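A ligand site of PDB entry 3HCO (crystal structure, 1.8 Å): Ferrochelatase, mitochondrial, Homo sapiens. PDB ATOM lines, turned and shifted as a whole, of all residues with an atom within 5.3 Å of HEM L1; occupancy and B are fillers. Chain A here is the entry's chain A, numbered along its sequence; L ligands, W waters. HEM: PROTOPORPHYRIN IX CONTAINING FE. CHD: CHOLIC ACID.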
ATOM      1  N   MET A  12      -5.151   6.489 -15.807  1.00  0.00           N
ATOM      2  CA  MET A  12      -6.090   6.096 -14.761  1.00  0.00           C
ATOM      3  C   MET A  12      -6.230   4.563 -14.725  1.00  0.00           C
ATOM      4  O   MET A  12      -6.725   3.995 -13.737  1.00  0.00           O
ATOM      5  CB  MET A  12      -7.490   6.708 -14.988  1.00  0.00           C
ATOM      6  CG  MET A  12      -8.084   6.295 -16.368  1.00  0.00           C
ATOM      7  SD  MET A  12      -9.726   6.927 -16.767  1.00  0.00           S
ATOM      8  CE  MET A  12     -10.722   6.474 -15.414  1.00  0.00           C
ATOM      9  N   PHE A  24     -11.839  -1.004  -9.379  1.00  0.00           N
ATOM     10  CA  PHE A  24     -11.576   0.188 -10.227  1.00  0.00           C
ATOM     11  C   PHE A  24     -12.430   1.360  -9.769  1.00  0.00           C
ATOM     12  O   PHE A  24     -11.916   2.451  -9.524  1.00  0.00           O
ATOM     13  CB  PHE A  24     -11.833  -0.151 -11.710  1.00  0.00           C
ATOM     14  CG  PHE A  24     -11.895   1.054 -12.640  1.00  0.00           C
ATOM     15  CD1 PHE A  24     -10.754   1.785 -12.924  1.00  0.00           C
ATOM     16  CD2 PHE A  24     -13.093   1.422 -13.230  1.00  0.00           C
ATOM     17  CE1 PHE A  24     -10.815   2.861 -13.770  1.00  0.00           C
ATOM     18  CE2 PHE A  24     -13.167   2.520 -14.110  1.00  0.00           C
ATOM     19  CZ  PHE A  24     -12.014   3.215 -14.378  1.00  0.00           C
ATOM     20  N   LEU A  25     -13.740   1.144  -9.627  1.00  0.00           N
ATOM     21  CA  LEU A  25     -14.670   2.175  -9.168  1.00  0.00           C
ATOM     22  C   LEU A  25     -14.458   2.636  -7.729  1.00  0.00           C
ATOM     23  O   LEU A  25     -14.585   3.820  -7.403  1.00  0.00           O
ATOM     24  CB  LEU A  25     -16.116   1.740  -9.337  1.00  0.00           C
ATOM     25  CG  LEU A  25     -16.695   1.575 -10.749  1.00  0.00           C
ATOM     26  CD1 LEU A  25     -18.174   1.207 -10.696  1.00  0.00           C
ATOM     27  CD2 LEU A  25     -16.522   2.901 -11.534  1.00  0.00           C
ATOM     28  N   LEU A  28     -11.559   4.932  -7.666  1.00  0.00           N
ATOM     29  CA  LEU A  28     -11.919   6.187  -8.361  1.00  0.00           C
ATOM     30  C   LEU A  28     -12.747   7.082  -7.452  1.00  0.00           C
ATOM     31  O   LEU A  28     -12.445   8.277  -7.238  1.00  0.00           O
ATOM     32  CB  LEU A  28     -12.665   5.846  -9.660  1.00  0.00           C
ATOM     33  CG  LEU A  28     -12.968   6.943 -10.676  1.00  0.00           C
ATOM     34  CD1 LEU A  28     -12.970   6.380 -12.119  1.00  0.00           C
ATOM     35  CD2 LEU A  28     -14.308   7.515 -10.311  1.00  0.00           C
ATOM     36  N   PHE A  29     -13.777   6.500  -6.839  1.00  0.00           N
ATOM     37  CA  PHE A  29     -14.623   7.297  -5.955  1.00  0.00           C
ATOM     38  C   PHE A  29     -13.925   7.681  -4.636  1.00  0.00           C
ATOM     39  O   PHE A  29     -14.352   8.631  -3.976  1.00  0.00           O
ATOM     40  CB  PHE A  29     -15.986   6.657  -5.766  1.00  0.00           C
ATOM     41  CG  PHE A  29     -16.889   6.803  -6.942  1.00  0.00           C
ATOM     42  CD1 PHE A  29     -17.132   5.725  -7.808  1.00  0.00           C
ATOM     43  CD2 PHE A  29     -17.513   8.012  -7.207  1.00  0.00           C
ATOM     44  CE1 PHE A  29     -17.980   5.863  -8.928  1.00  0.00           C
ATOM     45  CE2 PHE A  29     -18.368   8.179  -8.320  1.00  0.00           C
ATOM     46  CZ  PHE A  29     -18.599   7.093  -9.187  1.00  0.00           C
ATOM     47  N   LEU A  34      -9.602  13.720  -7.523  1.00  0.00           N
ATOM     48  CA  LEU A  34     -10.639  13.739  -8.529  1.00  0.00           C
ATOM     49  C   LEU A  34     -11.900  14.464  -8.060  1.00  0.00           C
ATOM     50  O   LEU A  34     -12.417  15.333  -8.762  1.00  0.00           O
ATOM     51  CB  LEU A  34     -11.033  12.309  -8.946  1.00  0.00           C
ATOM     52  CG  LEU A  34     -12.211  12.188  -9.939  1.00  0.00           C
ATOM     53  CD1 LEU A  34     -11.890  12.969 -11.224  1.00  0.00           C
ATOM     54  CD2 LEU A  34     -12.475  10.691 -10.251  1.00  0.00           C
ATOM     55  N   MET A  35     -12.428  14.078  -6.917  1.00  0.00           N
ATOM     56  CA  MET A  35     -13.693  14.648  -6.485  1.00  0.00           C
ATOM     57  C   MET A  35     -13.697  14.672  -4.983  1.00  0.00           C
ATOM     58  O   MET A  35     -12.952  13.914  -4.344  1.00  0.00           O
ATOM     59  CB  MET A  35     -14.885  13.819  -6.981  1.00  0.00           C
ATOM     60  CG  MET A  35     -14.861  12.360  -6.482  1.00  0.00           C
ATOM     61  SD  MET A  35     -16.262  11.350  -7.021  1.00  0.00           S
ATOM     62  CE  MET A  35     -15.926  11.142  -8.797  1.00  0.00           C
ATOM     63  N   ARG A  51     -22.805   1.318  -8.563  1.00  0.00           N
ATOM     64  CA  ARG A  51     -22.586   1.565  -9.999  1.00  0.00           C
ATOM     65  C   ARG A  51     -21.913   0.429 -10.762  1.00  0.00           C
ATOM     66  O   ARG A  51     -21.800   0.498 -11.990  1.00  0.00           O
ATOM     67  CB  ARG A  51     -21.758   2.844 -10.234  1.00  0.00           C
ATOM     68  CG  ARG A  51     -22.506   4.123  -9.933  1.00  0.00           C
ATOM     69  CD  ARG A  51     -21.647   5.373 -10.176  1.00  0.00           C
ATOM     70  NE  ARG A  51     -21.545   5.743 -11.600  1.00  0.00           N
ATOM     71  CZ  ARG A  51     -22.544   6.286 -12.292  1.00  0.00           C
ATOM     72  NH1 ARG A  51     -23.715   6.506 -11.719  1.00  0.00           N
ATOM     73  NH2 ARG A  51     -22.372   6.609 -13.574  1.00  0.00           N
ATOM     74  N   ILE A  55     -21.657  -0.096 -14.997  1.00  0.00           N
ATOM     75  CA  ILE A  55     -20.336  -0.006 -15.622  1.00  0.00           C
ATOM     76  C   ILE A  55     -19.827  -1.348 -16.205  1.00  0.00           C
ATOM     77  O   ILE A  55     -19.197  -1.389 -17.277  1.00  0.00           O
ATOM     78  CB  ILE A  55     -19.299   0.655 -14.667  1.00  0.00           C
ATOM     79  CG1 ILE A  55     -19.815   2.019 -14.176  1.00  0.00           C
ATOM     80  CG2 ILE A  55     -17.931   0.731 -15.328  1.00  0.00           C
ATOM     81  CD1 ILE A  55     -20.435   2.953 -15.313  1.00  0.00           C
ATOM     82  N   TYR A  59     -18.814  -1.898 -20.101  1.00  0.00           N
ATOM     83  CA  TYR A  59     -17.617  -2.551 -20.572  1.00  0.00           C
ATOM     84  C   TYR A  59     -17.913  -3.827 -21.440  1.00  0.00           C
ATOM     85  O   TYR A  59     -17.205  -4.103 -22.427  1.00  0.00           O
ATOM     86  CB  TYR A  59     -16.689  -2.904 -19.395  1.00  0.00           C
ATOM     87  CG  TYR A  59     -15.819  -1.749 -19.027  1.00  0.00           C
ATOM     88  CD1 TYR A  59     -16.032  -1.059 -17.836  1.00  0.00           C
ATOM     89  CD2 TYR A  59     -14.857  -1.260 -19.928  1.00  0.00           C
ATOM     90  CE1 TYR A  59     -15.249   0.049 -17.501  1.00  0.00           C
ATOM     91  CE2 TYR A  59     -14.066  -0.139 -19.599  1.00  0.00           C
ATOM     92  CZ  TYR A  59     -14.259   0.488 -18.397  1.00  0.00           C
ATOM     93  OH  TYR A  59     -13.513   1.602 -18.061  1.00  0.00           O
ATOM     94  N   TYR A 127      -1.928  11.289 -20.593  1.00  0.00           N
ATOM     95  CA  TYR A 127      -2.947  12.225 -21.063  1.00  0.00           C
ATOM     96  C   TYR A 127      -2.265  13.414 -21.723  1.00  0.00           C
ATOM     97  O   TYR A 127      -1.525  14.162 -21.029  1.00  0.00           O
ATOM     98  CB  TYR A 127      -3.700  12.810 -19.856  1.00  0.00           C
ATOM     99  CG  TYR A 127      -4.354  11.799 -18.911  1.00  0.00           C
ATOM    100  CD1 TYR A 127      -3.681  11.352 -17.756  1.00  0.00           C
ATOM    101  CD2 TYR A 127      -5.675  11.356 -19.148  1.00  0.00           C
ATOM    102  CE1 TYR A 127      -4.320  10.504 -16.809  1.00  0.00           C
ATOM    103  CE2 TYR A 127      -6.312  10.473 -18.230  1.00  0.00           C
ATOM    104  CZ  TYR A 127      -5.602  10.061 -17.076  1.00  0.00           C
ATOM    105  OH  TYR A 127      -6.184   9.240 -16.153  1.00  0.00           O
ATOM    106  N   SER A 131      -5.373  17.965 -17.060  1.00  0.00           N
ATOM    107  CA  SER A 131      -6.470  18.312 -16.140  1.00  0.00           C
ATOM    108  C   SER A 131      -5.987  17.983 -14.723  1.00  0.00           C
ATOM    109  O   SER A 131      -5.270  17.028 -14.486  1.00  0.00           O
ATOM    110  CB  SER A 131      -7.761  17.565 -16.435  1.00  0.00           C
ATOM    111  OG  SER A 131      -8.770  17.875 -15.450  1.00  0.00           O
ATOM    112  N   SER A 133      -7.795  16.675 -12.700  1.00  0.00           N
ATOM    113  CA  SER A 133      -8.534  15.414 -12.381  1.00  0.00           C
ATOM    114  C   SER A 133      -7.801  14.181 -12.900  1.00  0.00           C
ATOM    115  O   SER A 133      -8.072  13.074 -12.460  1.00  0.00           O
ATOM    116  CB  SER A 133      -9.929  15.452 -12.948  1.00  0.00           C
ATOM    117  OG  SER A 133      -9.971  15.484 -14.379  1.00  0.00           O
ATOM    118  N   THR A 134      -6.906  14.383 -13.873  1.00  0.00           N
ATOM    119  CA  THR A 134      -6.287  13.260 -14.559  1.00  0.00           C
ATOM    120  C   THR A 134      -4.809  13.296 -14.231  1.00  0.00           C
ATOM    121  O   THR A 134      -4.377  12.679 -13.227  1.00  0.00           O
ATOM    122  CB  THR A 134      -6.631  13.278 -16.091  1.00  0.00           C
ATOM    123  OG1 THR A 134      -6.234  14.547 -16.630  1.00  0.00           O
ATOM    124  CG2 THR A 134      -8.139  13.041 -16.260  1.00  0.00           C
ATOM    125  N   HIS A 199     -13.649  13.785 -23.112  1.00  0.00           N
ATOM    126  CA  HIS A 199     -14.452  13.663 -21.886  1.00  0.00           C
ATOM    127  C   HIS A 199     -14.678  15.049 -21.260  1.00  0.00           C
ATOM    128  O   HIS A 199     -13.775  15.875 -21.130  1.00  0.00           O
ATOM    129  CB  HIS A 199     -13.730  12.758 -20.880  1.00  0.00           C
ATOM    130  CG  HIS A 199     -13.811  11.308 -21.215  1.00  0.00           C
ATOM    131  ND1 HIS A 199     -12.933  10.687 -22.092  1.00  0.00           N
ATOM    132  CD2 HIS A 199     -14.669  10.352 -20.788  1.00  0.00           C
ATOM    133  CE1 HIS A 199     -13.257   9.406 -22.184  1.00  0.00           C
ATOM    134  NE2 HIS A 199     -14.318   9.190 -21.415  1.00  0.00           N
ATOM    135  N   SER A 200     -15.919  15.315 -20.845  1.00  0.00           N
ATOM    136  CA  SER A 200     -16.235  16.561 -20.189  1.00  0.00           C
ATOM    137  C   SER A 200     -15.644  16.733 -18.796  1.00  0.00           C
ATOM    138  O   SER A 200     -15.123  15.767 -18.171  1.00  0.00           O
ATOM    139  CB  SER A 200     -17.794  16.698 -20.229  1.00  0.00           C
ATOM    140  OG  SER A 200     -18.175  17.991 -19.807  1.00  0.00           O
ATOM    141  N   LEU A 201     -15.716  17.956 -18.281  1.00  0.00           N
ATOM    142  CA  LEU A 201     -15.477  18.282 -16.873  1.00  0.00           C
ATOM    143  C   LEU A 201     -16.760  18.921 -16.283  1.00  0.00           C
ATOM    144  O   LEU A 201     -17.492  19.623 -16.987  1.00  0.00           O
ATOM    145  CB  LEU A 201     -14.355  19.324 -16.752  1.00  0.00           C
ATOM    146  CG  LEU A 201     -12.968  18.880 -17.238  1.00  0.00           C
ATOM    147  CD1 LEU A 201     -12.027  20.088 -17.109  1.00  0.00           C
ATOM    148  CD2 LEU A 201     -12.437  17.685 -16.450  1.00  0.00           C
ATOM    149  N   PRO A 202     -16.982  18.704 -14.969  1.00  0.00           N
ATOM    150  CA  PRO A 202     -18.024  19.450 -14.292  1.00  0.00           C
ATOM    151  C   PRO A 202     -17.741  20.955 -14.419  1.00  0.00           C
ATOM    152  O   PRO A 202     -16.576  21.368 -14.340  1.00  0.00           O
ATOM    153  CB  PRO A 202     -17.855  19.005 -12.809  1.00  0.00           C
ATOM    154  CG  PRO A 202     -17.227  17.660 -12.870  1.00  0.00           C
ATOM    155  CD  PRO A 202     -16.272  17.758 -14.078  1.00  0.00           C
ATOM    156  N   VAL A 205     -15.417  22.520 -12.000  1.00  0.00           N
ATOM    157  CA  VAL A 205     -13.968  22.282 -12.172  1.00  0.00           C
ATOM    158  C   VAL A 205     -13.459  23.227 -13.275  1.00  0.00           C
ATOM    159  O   VAL A 205     -12.371  23.837 -13.115  1.00  0.00           O
ATOM    160  CB  VAL A 205     -13.703  20.820 -12.564  1.00  0.00           C
ATOM    161  CG1 VAL A 205     -12.225  20.612 -12.864  1.00  0.00           C
ATOM    162  CG2 VAL A 205     -14.165  19.895 -11.399  1.00  0.00           C
ATOM    163  N   TYR A 212      -7.520  22.044 -18.797  1.00  0.00           N
ATOM    164  CA  TYR A 212      -7.858  21.027 -19.838  1.00  0.00           C
ATOM    165  C   TYR A 212      -8.635  21.526 -21.081  1.00  0.00           C
ATOM    166  O   TYR A 212      -8.213  21.235 -22.180  1.00  0.00           O
ATOM    167  CB  TYR A 212      -8.551  19.830 -19.143  1.00  0.00           C
ATOM    168  CG  TYR A 212      -9.267  18.744 -19.954  1.00  0.00           C
ATOM    169  CD1 TYR A 212      -8.553  17.623 -20.366  1.00  0.00           C
ATOM    170  CD2 TYR A 212     -10.651  18.776 -20.175  1.00  0.00           C
ATOM    171  CE1 TYR A 212      -9.182  16.547 -21.012  1.00  0.00           C
ATOM    172  CE2 TYR A 212     -11.313  17.715 -20.848  1.00  0.00           C
ATOM    173  CZ  TYR A 212     -10.533  16.607 -21.256  1.00  0.00           C
ATOM    174  OH  TYR A 212     -11.128  15.544 -21.857  1.00  0.00           O
ATOM    175  N   SER A 239     -19.585  11.696 -22.333  1.00  0.00           N
ATOM    176  CA  SER A 239     -19.705  10.857 -21.131  1.00  0.00           C
ATOM    177  C   SER A 239     -20.011  11.560 -19.780  1.00  0.00           C
ATOM    178  O   SER A 239     -19.801  10.966 -18.722  1.00  0.00           O
ATOM    179  CB  SER A 239     -18.487   9.911 -21.060  1.00  0.00           C
ATOM    180  OG  SER A 239     -18.189   9.384 -22.338  1.00  0.00           O
ATOM    181  N   VAL A 241     -21.110  12.536 -16.313  1.00  0.00           N
ATOM    182  CA  VAL A 241     -21.793  11.681 -15.341  1.00  0.00           C
ATOM    183  C   VAL A 241     -22.667  12.475 -14.294  1.00  0.00           C
ATOM    184  O   VAL A 241     -22.203  13.455 -13.668  1.00  0.00           O
ATOM    185  CB  VAL A 241     -20.809  10.595 -14.751  1.00  0.00           C
ATOM    186  CG1 VAL A 241     -20.499   9.548 -15.813  1.00  0.00           C
ATOM    187  CG2 VAL A 241     -19.501  11.232 -14.267  1.00  0.00           C
ATOM    188  N   TRP A 246     -22.204  20.145 -16.537  1.00  0.00           N
ATOM    189  CA  TRP A 246     -20.891  19.788 -17.071  1.00  0.00           C
ATOM    190  C   TRP A 246     -20.684  20.613 -18.357  1.00  0.00           C
ATOM    191  O   TRP A 246     -21.635  21.147 -18.936  1.00  0.00           O
ATOM    192  CB  TRP A 246     -20.834  18.294 -17.423  1.00  0.00           C
ATOM    193  CG  TRP A 246     -20.674  17.387 -16.230  1.00  0.00           C
ATOM    194  CD1 TRP A 246     -21.577  17.248 -15.170  1.00  0.00           C
ATOM    195  CD2 TRP A 246     -19.605  16.440 -15.975  1.00  0.00           C
ATOM    196  NE1 TRP A 246     -21.104  16.292 -14.277  1.00  0.00           N
ATOM    197  CE2 TRP A 246     -19.930  15.766 -14.746  1.00  0.00           C
ATOM    198  CE3 TRP A 246     -18.435  16.074 -16.666  1.00  0.00           C
ATOM    199  CZ2 TRP A 246     -19.084  14.796 -14.189  1.00  0.00           C
ATOM    200  CZ3 TRP A 246     -17.589  15.075 -16.076  1.00  0.00           C
ATOM    201  CH2 TRP A 246     -17.938  14.458 -14.862  1.00  0.00           C
ATOM    202  N   ALA A 272      -8.851  13.173 -26.663  1.00  0.00           N
ATOM    203  CA  ALA A 272      -8.243  13.430 -25.297  1.00  0.00           C
ATOM    204  C   ALA A 272      -8.064  12.155 -24.493  1.00  0.00           C
ATOM    205  O   ALA A 272      -7.675  12.186 -23.350  1.00  0.00           O
ATOM    206  CB  ALA A 272      -9.080  14.440 -24.467  1.00  0.00           C
ATOM    207  N   PHE A 273      -8.284  11.002 -25.113  1.00  0.00           N
ATOM    208  CA  PHE A 273      -8.001   9.754 -24.387  1.00  0.00           C
ATOM    209  C   PHE A 273      -7.657   8.720 -25.422  1.00  0.00           C
ATOM    210  O   PHE A 273      -8.474   8.479 -26.335  1.00  0.00           O
ATOM    211  CB  PHE A 273      -9.167   9.325 -23.508  1.00  0.00           C
ATOM    212  CG  PHE A 273      -8.820   8.264 -22.532  1.00  0.00           C
ATOM    213  CD1 PHE A 273      -8.252   8.602 -21.303  1.00  0.00           C
ATOM    214  CD2 PHE A 273      -9.020   6.914 -22.827  1.00  0.00           C
ATOM    215  CE1 PHE A 273      -7.885   7.647 -20.384  1.00  0.00           C
ATOM    216  CE2 PHE A 273      -8.636   5.930 -21.886  1.00  0.00           C
ATOM    217  CZ  PHE A 273      -8.076   6.325 -20.666  1.00  0.00           C
ATOM    218  N   HIS A 277     -12.318   3.226 -25.137  1.00  0.00           N
ATOM    219  CA  HIS A 277     -13.034   3.541 -23.912  1.00  0.00           C
ATOM    220  C   HIS A 277     -14.539   3.440 -24.160  1.00  0.00           C
ATOM    221  O   HIS A 277     -14.960   3.062 -25.262  1.00  0.00           O
ATOM    222  CB  HIS A 277     -12.600   4.932 -23.359  1.00  0.00           C
ATOM    223  CG  HIS A 277     -12.669   6.047 -24.365  1.00  0.00           C
ATOM    224  ND1 HIS A 277     -11.640   6.301 -25.243  1.00  0.00           N
ATOM    225  CD2 HIS A 277     -13.615   6.991 -24.590  1.00  0.00           C
ATOM    226  CE1 HIS A 277     -11.960   7.351 -25.983  1.00  0.00           C
ATOM    227  NE2 HIS A 277     -13.147   7.780 -25.614  1.00  0.00           N
ATOM    228  N   ILE A 278     -15.356   3.725 -23.152  1.00  0.00           N
ATOM    229  CA  ILE A 278     -16.797   3.559 -23.317  1.00  0.00           C
ATOM    230  C   ILE A 278     -17.349   4.504 -24.363  1.00  0.00           C
ATOM    231  O   ILE A 278     -16.993   5.680 -24.377  1.00  0.00           O
ATOM    232  CB  ILE A 278     -17.593   3.703 -21.983  1.00  0.00           C
ATOM    233  CG1 ILE A 278     -17.184   2.591 -20.976  1.00  0.00           C
ATOM    234  CG2 ILE A 278     -19.095   3.597 -22.277  1.00  0.00           C
ATOM    235  CD1 ILE A 278     -17.770   2.795 -19.596  1.00  0.00           C
HETATM  236  CHA HEM L   1     -14.612   7.131 -15.716  1.00  0.00           C
HETATM  237  CHB HEM L   1     -15.812  11.118 -13.302  1.00  0.00           C
HETATM  238  CHC HEM L   1     -12.555  13.729 -15.817  1.00  0.00           C
HETATM  239  CHD HEM L   1     -11.865   9.927 -18.673  1.00  0.00           C
HETATM  240  C1A HEM L   1     -15.195   7.966 -14.816  1.00  0.00           C
HETATM  241  C2A HEM L   1     -16.066   7.565 -13.761  1.00  0.00           C
HETATM  242  C3A HEM L   1     -16.415   8.669 -13.066  1.00  0.00           C
HETATM  243  C4A HEM L   1     -15.749   9.815 -13.679  1.00  0.00           C
HETATM  244  CMA HEM L   1     -17.363   8.733 -11.850  1.00  0.00           C
HETATM  245  CAA HEM L   1     -16.467   6.089 -13.525  1.00  0.00           C
HETATM  246  CBA HEM L   1     -17.590   5.640 -14.444  1.00  0.00           C
HETATM  247  CGA HEM L   1     -18.896   6.060 -13.834  1.00  0.00           C
HETATM  248  O1A HEM L   1     -19.740   6.538 -14.619  1.00  0.00           O
HETATM  249  O2A HEM L   1     -19.124   5.893 -12.594  1.00  0.00           O
HETATM  250  C1B HEM L   1     -14.977  12.131 -13.727  1.00  0.00           C
HETATM  251  C2B HEM L   1     -14.877  13.428 -13.101  1.00  0.00           C
HETATM  252  C3B HEM L   1     -13.949  14.147 -13.765  1.00  0.00           C
HETATM  253  C4B HEM L   1     -13.482  13.324 -14.869  1.00  0.00           C
HETATM  254  CMB HEM L   1     -15.680  13.871 -11.843  1.00  0.00           C
HETATM  255  CAB HEM L   1     -13.503  15.607 -13.512  1.00  0.00           C
HETATM  256  CBB HEM L   1     -13.467  16.229 -12.306  1.00  0.00           C
HETATM  257  C1C HEM L   1     -12.110  12.962 -16.867  1.00  0.00           C
HETATM  258  C2C HEM L   1     -11.184  13.378 -17.964  1.00  0.00           C
HETATM  259  C3C HEM L   1     -10.999  12.292 -18.729  1.00  0.00           C
HETATM  260  C4C HEM L   1     -11.781  11.190 -18.151  1.00  0.00           C
HETATM  261  CMC HEM L   1     -10.638  14.806 -18.026  1.00  0.00           C
HETATM  262  CAC HEM L   1     -10.174  12.082 -20.024  1.00  0.00           C
HETATM  263  CBC HEM L   1      -9.029  12.677 -20.236  1.00  0.00           C
HETATM  264  C1D HEM L   1     -12.529   8.846 -18.139  1.00  0.00           C
HETATM  265  C2D HEM L   1     -12.464   7.517 -18.678  1.00  0.00           C
HETATM  266  C3D HEM L   1     -13.311   6.665 -17.724  1.00  0.00           C
HETATM  267  C4D HEM L   1     -13.797   7.561 -16.746  1.00  0.00           C
HETATM  268  CMD HEM L   1     -11.690   7.053 -19.925  1.00  0.00           C
HETATM  269  CAD HEM L   1     -13.599   5.149 -17.753  1.00  0.00           C
HETATM  270  CBD HEM L   1     -14.908   4.740 -18.371  1.00  0.00           C
HETATM  271  CGD HEM L   1     -15.009   5.198 -19.798  1.00  0.00           C
HETATM  272  O1D HEM L   1     -14.323   4.630 -20.680  1.00  0.00           O
HETATM  273  O2D HEM L   1     -15.738   6.189 -20.035  1.00  0.00           O
HETATM  274  NA  HEM L   1     -14.989   9.326 -14.712  1.00  0.00           N
HETATM  275  NB  HEM L   1     -14.119  12.073 -14.813  1.00  0.00           N
HETATM  276  NC  HEM L   1     -12.441  11.648 -17.053  1.00  0.00           N
HETATM  277  ND  HEM L   1     -13.354   8.846 -16.992  1.00  0.00           N
HETATM  278 FE   HEM L   1     -13.720  10.502 -15.922  1.00  0.00          FE
HETATM  279  C1  CHD L   2     -19.059  17.856  -9.873  1.00  0.00           C
HETATM  280  C2  CHD L   2     -20.034  18.923  -9.407  1.00  0.00           C
HETATM  281  C3  CHD L   2     -19.485  19.630  -8.170  1.00  0.00           C
HETATM  282  O3  CHD L   2     -20.429  20.612  -7.729  1.00  0.00           O
HETATM  283  C4  CHD L   2     -19.238  18.624  -7.046  1.00  0.00           C
HETATM  284  C5  CHD L   2     -18.283  17.477  -7.438  1.00  0.00           C
HETATM  285  C6  CHD L   2     -18.203  16.452  -6.285  1.00  0.00           C
HETATM  286  C7  CHD L   2     -19.215  15.287  -6.360  1.00  0.00           C
HETATM  287  O7  CHD L   2     -20.543  15.762  -6.078  1.00  0.00           O
HETATM  288  C8  CHD L   2     -19.216  14.625  -7.735  1.00  0.00           C
HETATM  289  C9  CHD L   2     -19.612  15.730  -8.725  1.00  0.00           C
HETATM  290  C10 CHD L   2     -18.562  16.847  -8.832  1.00  0.00           C
HETATM  291  C11 CHD L   2     -20.117  15.202 -10.087  1.00  0.00           C
HETATM  292  C12 CHD L   2     -21.087  14.026  -9.973  1.00  0.00           C
HETATM  293  O12 CHD L   2     -22.310  14.415  -9.337  1.00  0.00           O
HETATM  294  C13 CHD L   2     -20.421  12.879  -9.223  1.00  0.00           C
HETATM  295  C14 CHD L   2     -20.147  13.402  -7.819  1.00  0.00           C
HETATM  296  C15 CHD L   2     -19.800  12.145  -7.008  1.00  0.00           C
HETATM  297  C16 CHD L   2     -20.882  11.103  -7.541  1.00  0.00           C
HETATM  298  C17 CHD L   2     -21.323  11.677  -8.920  1.00  0.00           C
HETATM  299  C18 CHD L   2     -19.105  12.510  -9.936  1.00  0.00           C
HETATM  300  C19 CHD L   2     -17.217  16.291  -9.324  1.00  0.00           C
HETATM  301  C20 CHD L   2     -21.578  10.568  -9.983  1.00  0.00           C
HETATM  302  C21 CHD L   2     -20.462  10.271 -10.977  1.00  0.00           C
HETATM  303  C22 CHD L   2     -22.865  10.841 -10.757  1.00  0.00           C
HETATM  304  C23 CHD L   2     -23.879   9.734 -10.519  1.00  0.00           C
HETATM  305  O25 CHD L   2     -26.004  10.583 -11.175  1.00  0.00           O
HETATM  306  C24 CHD L   2     -25.008   9.888 -11.514  1.00  0.00           C
HETATM  307  O26 CHD L   2     -24.905   9.340 -12.636  1.00  0.00           O
HETATM  308  O   HOH W   1     -16.455   7.270 -22.229  1.00  0.00           O
HETATM  309  O   HOH W   2     -12.315   2.781 -20.193  1.00  0.00           O
HETATM  310  O   HOH W   3     -11.187  12.253 -23.368  1.00  0.00           O
HETATM  311  O   HOH W   4      -6.613  14.978 -19.204  1.00  0.00           O
HETATM  312  O   HOH W   5     -19.715   6.053 -17.286  1.00  0.00           O
HETATM  313  O   HOH W   6     -17.745   7.452 -18.515  1.00  0.00           O
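OG1 of Thr 134 sits close to O of Ser 131, 3.4 Å away.
The backbone NH (N) of Met 12 lies within hydrogen-bond range of the side-chain hydroxyl (OH) of Tyr 127 (3.0 Å).
OH of Tyr 212 lies within hydrogen-bond range of O of His 199.
The backbone carbonyl oxygen of Val 241 lies within hydrogen-bond range of the indole nitrogen of Trp 246 (3.1 Å).
OG of Ser 133 lies within hydrogen-bond range of OG of Ser 131 (2.9 Å).
The backbone NH (N) of Ile 278 is in hydrogen-bond range of an oxygen (O1D) of HEM L1 (2.8 Å).
The guanidinium group (NE) of Arg 51 is in salt-bridge range of an oxygen (O2A) of HEM L1, 2.6 Å away.
NH1 of Arg 51 is in salt-bridge range of O26 of CHD L2, 3.2 Å away.
Residues that only touch HEM L1: Met 12, Leu 25, Leu 28, Phe 29, Leu 34, Ile 55, Tyr 59, Tyr 127, Ser 133, Thr 134, His 199, Leu 201, Pro 202, Val 205, Tyr 212, Val 241, Trp 246, Ala 272, Phe 273 and His 277.
Hydrophobic or aromatic side chains within 4 Å of HEM L1: Met 12, Leu 25, Leu 28, Phe 29, Leu 34, Ile 55, Tyr 127, His 199, Leu 201, Pro 202, Val 205, Tyr 212, Val 241, Trp 246, Phe 273, His 277 and Ile 278.
Within 4 Å of HEM L1: Met 12, Leu 25, Leu 28, Phe 29, Leu 34, Arg 51, Ile 55, Tyr 59, Tyr 127, Ser 133, Thr 134, His 199, Leu 201, Pro 202, Val 205, Tyr 212, Val 241, Trp 246, Ala 272, Phe 273, His 277 and Ile 278.
The nearest printed residue that does not touch HEM L1 is Ser 200 (4.04 Å).
Water W1 lies within hydrogen-bond range of an oxygen (O2D) of HEM L1, the backbone carbonyl oxygen (O) of Ile 278, the side-chain hydroxyl (OG) of Ser 239 and a ring nitrogen (NE2) of His 199.
Water W2 lies within hydrogen-bond range of OH of Tyr 59 (2.7 Å) and O1D of HEM L1 (2.8 Å).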
